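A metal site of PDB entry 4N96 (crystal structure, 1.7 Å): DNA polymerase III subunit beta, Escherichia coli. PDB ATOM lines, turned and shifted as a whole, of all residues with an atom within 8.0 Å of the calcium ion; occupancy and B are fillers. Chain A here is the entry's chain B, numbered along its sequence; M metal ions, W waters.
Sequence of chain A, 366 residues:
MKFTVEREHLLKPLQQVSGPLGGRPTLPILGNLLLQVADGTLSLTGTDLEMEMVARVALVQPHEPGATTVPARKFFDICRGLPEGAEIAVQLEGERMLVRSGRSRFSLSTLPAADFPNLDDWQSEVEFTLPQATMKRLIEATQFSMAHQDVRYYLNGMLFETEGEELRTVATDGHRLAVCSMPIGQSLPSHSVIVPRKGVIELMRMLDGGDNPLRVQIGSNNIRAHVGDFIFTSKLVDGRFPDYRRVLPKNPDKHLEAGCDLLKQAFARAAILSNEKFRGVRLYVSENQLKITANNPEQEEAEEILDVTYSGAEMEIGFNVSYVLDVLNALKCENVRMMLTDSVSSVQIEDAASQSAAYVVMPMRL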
ATOM      1  N   VAL A   5       7.837  -4.333 -22.966  1.00  0.00           N
ATOM      2  CA  VAL A   5       6.672  -5.087 -23.495  1.00  0.00           C
ATOM      3  C   VAL A   5       5.959  -5.826 -22.371  1.00  0.00           C
ATOM      4  O   VAL A   5       6.606  -6.384 -21.483  1.00  0.00           O
ATOM      5  CB  VAL A   5       7.101  -6.085 -24.595  1.00  0.00           C
ATOM      6  CG1 VAL A   5       5.933  -6.943 -25.079  1.00  0.00           C
ATOM      7  CG2 VAL A   5       7.684  -5.347 -25.791  1.00  0.00           C
ATOM      8  N   GLU A   6       4.626  -5.842 -22.419  1.00  0.00           N
ATOM      9  CA  GLU A   6       3.852  -6.593 -21.438  1.00  0.00           C
ATOM     10  C   GLU A   6       4.130  -8.083 -21.576  1.00  0.00           C
ATOM     11  O   GLU A   6       4.227  -8.618 -22.685  1.00  0.00           O
ATOM     12  CB  GLU A   6       2.342  -6.348 -21.549  1.00  0.00           C
ATOM     13  CG  GLU A   6       1.614  -6.780 -20.263  1.00  0.00           C
ATOM     14  CD  GLU A   6       0.218  -6.178 -20.091  1.00  0.00           C
ATOM     15  OE1 GLU A   6      -0.516  -6.116 -21.084  1.00  0.00           O
ATOM     16  OE2 GLU A   6      -0.133  -5.781 -18.935  1.00  0.00           O
ATOM     17  N   ARG A   7       4.253  -8.737 -20.436  1.00  0.00           N
ATOM     18  CA  ARG A   7       4.646 -10.142 -20.347  1.00  0.00           C
ATOM     19  C   ARG A   7       3.970 -11.012 -21.395  1.00  0.00           C
ATOM     20  O   ARG A   7       4.632 -11.752 -22.101  1.00  0.00           O
ATOM     21  CB  ARG A   7       4.308 -10.700 -18.960  1.00  0.00           C
ATOM     22  CG  ARG A   7       4.601 -12.172 -18.751  1.00  0.00           C
ATOM     23  CD  ARG A   7       4.256 -12.578 -17.331  1.00  0.00           C
ATOM     24  NE  ARG A   7       4.298 -14.038 -17.166  1.00  0.00           N
ATOM     25  CZ  ARG A   7       3.275 -14.866 -17.313  1.00  0.00           C
ATOM     26  NH1 ARG A   7       2.050 -14.443 -17.648  1.00  0.00           N
ATOM     27  NH2 ARG A   7       3.476 -16.180 -17.148  1.00  0.00           N
ATOM     28  N   GLU A   8       2.646 -10.937 -21.490  1.00  0.00           N
ATOM     29  CA  GLU A   8       1.908 -11.906 -22.291  1.00  0.00           C
ATOM     30  C   GLU A   8       2.033 -11.707 -23.793  1.00  0.00           C
ATOM     31  O   GLU A   8       1.745 -12.617 -24.559  1.00  0.00           O
ATOM     32  CB  GLU A   8       0.434 -11.994 -21.882  1.00  0.00           C
ATOM     33  CG  GLU A   8       0.224 -12.484 -20.447  1.00  0.00           C
ATOM     34  CD  GLU A   8       0.618 -11.462 -19.397  1.00  0.00           C
ATOM     35  OE1 GLU A   8       0.604 -10.255 -19.665  1.00  0.00           O
ATOM     36  OE2 GLU A   8       0.950 -11.878 -18.276  1.00  0.00           O
ATOM     37  N   GLN A  61       5.130   0.785 -26.690  1.00  0.00           N
ATOM     38  CA  GLN A  61       5.803   1.577 -25.663  1.00  0.00           C
ATOM     39  C   GLN A  61       7.105   2.104 -26.236  1.00  0.00           C
ATOM     40  O   GLN A  61       7.585   1.577 -27.250  1.00  0.00           O
ATOM     41  CB  GLN A  61       6.069   0.699 -24.456  1.00  0.00           C
ATOM     42  CG  GLN A  61       4.816   0.125 -23.822  1.00  0.00           C
ATOM     43  CD  GLN A  61       5.085  -0.590 -22.509  1.00  0.00           C
ATOM     44  OE1 GLN A  61       5.525   0.034 -21.546  1.00  0.00           O
ATOM     45  NE2 GLN A  61       4.784  -1.883 -22.457  1.00  0.00           N
ATOM     46  N   PRO A  83       5.038 -11.923 -12.794  1.00  0.00           N
ATOM     47  CA  PRO A  83       3.597 -11.909 -12.540  1.00  0.00           C
ATOM     48  C   PRO A  83       2.805 -11.499 -13.774  1.00  0.00           C
ATOM     49  O   PRO A  83       3.310 -10.777 -14.621  1.00  0.00           O
ATOM     50  CB  PRO A  83       3.459 -10.893 -11.410  1.00  0.00           C
ATOM     51  CG  PRO A  83       4.622  -9.987 -11.531  1.00  0.00           C
ATOM     52  CD  PRO A  83       5.741 -10.881 -12.024  1.00  0.00           C
ATOM     53  N   GLU A  84       1.586 -12.018 -13.876  1.00  0.00           N
ATOM     54  CA  GLU A  84       0.720 -11.705 -14.976  1.00  0.00           C
ATOM     55  C   GLU A  84       0.620 -10.182 -15.176  1.00  0.00           C
ATOM     56  O   GLU A  84       0.457  -9.436 -14.216  1.00  0.00           O
ATOM     57  CB  GLU A  84      -0.675 -12.271 -14.702  1.00  0.00           C
ATOM     58  CG  GLU A  84      -1.614 -12.179 -15.867  1.00  0.00           C
ATOM     59  CD  GLU A  84      -2.645 -13.268 -15.844  1.00  0.00           C
ATOM     60  OE1 GLU A  84      -3.017 -13.684 -14.735  1.00  0.00           O
ATOM     61  OE2 GLU A  84      -3.058 -13.718 -16.920  1.00  0.00           O
ATOM     62  N   GLY A  85       0.748  -9.744 -16.421  1.00  0.00           N
ATOM     63  CA  GLY A  85       0.689  -8.316 -16.764  1.00  0.00           C
ATOM     64  C   GLY A  85       1.967  -7.523 -16.453  1.00  0.00           C
ATOM     65  O   GLY A  85       1.970  -6.301 -16.581  1.00  0.00           O
ATOM     66  N   ALA A  86       3.010  -8.215 -16.014  1.00  0.00           N
ATOM     67  CA  ALA A  86       4.322  -7.606 -15.746  1.00  0.00           C
ATOM     68  C   ALA A  86       4.810  -6.855 -16.983  1.00  0.00           C
ATOM     69  O   ALA A  86       4.805  -7.411 -18.089  1.00  0.00           O
ATOM     70  CB  ALA A  86       5.348  -8.694 -15.411  1.00  0.00           C
ATOM     71  N   GLU A  87       5.259  -5.614 -16.801  1.00  0.00           N
ATOM     72  CA  GLU A  87       5.925  -4.875 -17.871  1.00  0.00           C
ATOM     73  C   GLU A  87       7.390  -5.283 -17.854  1.00  0.00           C
ATOM     74  O   GLU A  87       8.039  -5.186 -16.821  1.00  0.00           O
ATOM     75  CB  GLU A  87       5.797  -3.370 -17.634  1.00  0.00           C
ATOM     76  CG  GLU A  87       4.362  -2.912 -17.546  1.00  0.00           C
ATOM     77  CD  GLU A  87       3.554  -3.206 -18.794  1.00  0.00           C
ATOM     78  OE1 GLU A  87       4.113  -3.204 -19.916  1.00  0.00           O
ATOM     79  OE2 GLU A  87       2.342  -3.433 -18.664  1.00  0.00           O
ATOM     80  N   ILE A  88       7.883  -5.770 -18.989  1.00  0.00           N
ATOM     81  CA  ILE A  88       9.237  -6.290 -19.103  1.00  0.00           C
ATOM     82  C   ILE A  88      10.081  -5.290 -19.878  1.00  0.00           C
ATOM     83  O   ILE A  88       9.892  -5.100 -21.098  1.00  0.00           O
ATOM     84  CB  ILE A  88       9.238  -7.671 -19.782  1.00  0.00           C
ATOM     85  CG1 ILE A  88       8.215  -8.569 -19.081  1.00  0.00           C
ATOM     86  CG2 ILE A  88      10.636  -8.282 -19.708  1.00  0.00           C
ATOM     87  CD1 ILE A  88       8.336 -10.054 -19.309  1.00  0.00           C
ATOM     88  N   SER A 101      11.606  -5.720 -14.288  1.00  0.00           N
ATOM     89  CA  SER A 101      10.164  -5.656 -14.167  1.00  0.00           C
ATOM     90  C   SER A 101       9.840  -5.538 -12.683  1.00  0.00           C
ATOM     91  O   SER A 101      10.270  -6.373 -11.879  1.00  0.00           O
ATOM     92  CB  SER A 101       9.479  -6.922 -14.705  1.00  0.00           C
ATOM     93  OG  SER A 101       8.066  -6.803 -14.636  1.00  0.00           O
HETATM   94 CA    CA M   1       0.867  -4.354 -17.041  1.00  0.00          CA
HETATM   95  O   HOH W   1      -0.127  -2.263 -17.501  1.00  0.00           O
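OE1 of Glu 87 lies within hydrogen-bond range of NE2 of Gln 61 (2.9 Å).
OG of Ser 101 lies within hydrogen-bond range of O of Glu 87, 2.7 Å away.
N of Gly 85 sits at hydrogen-bond distance from OE2 of Glu 8, at 2.8 Å.
Three residues have an atom within 4 Å of the calcium ion: Glu 6, Gly 85 and Glu 87.
The calcium ion is bound by the backbone carbonyl oxygen of Gly 85 (2.3 Å), water W1 (2.4 Å), the side-chain carboxylate of Glu 87 (2.4 Å) and the side-chain carboxylate of Glu 6 (2.6 Å).
The calcium ion has four donor atoms within binding distance.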
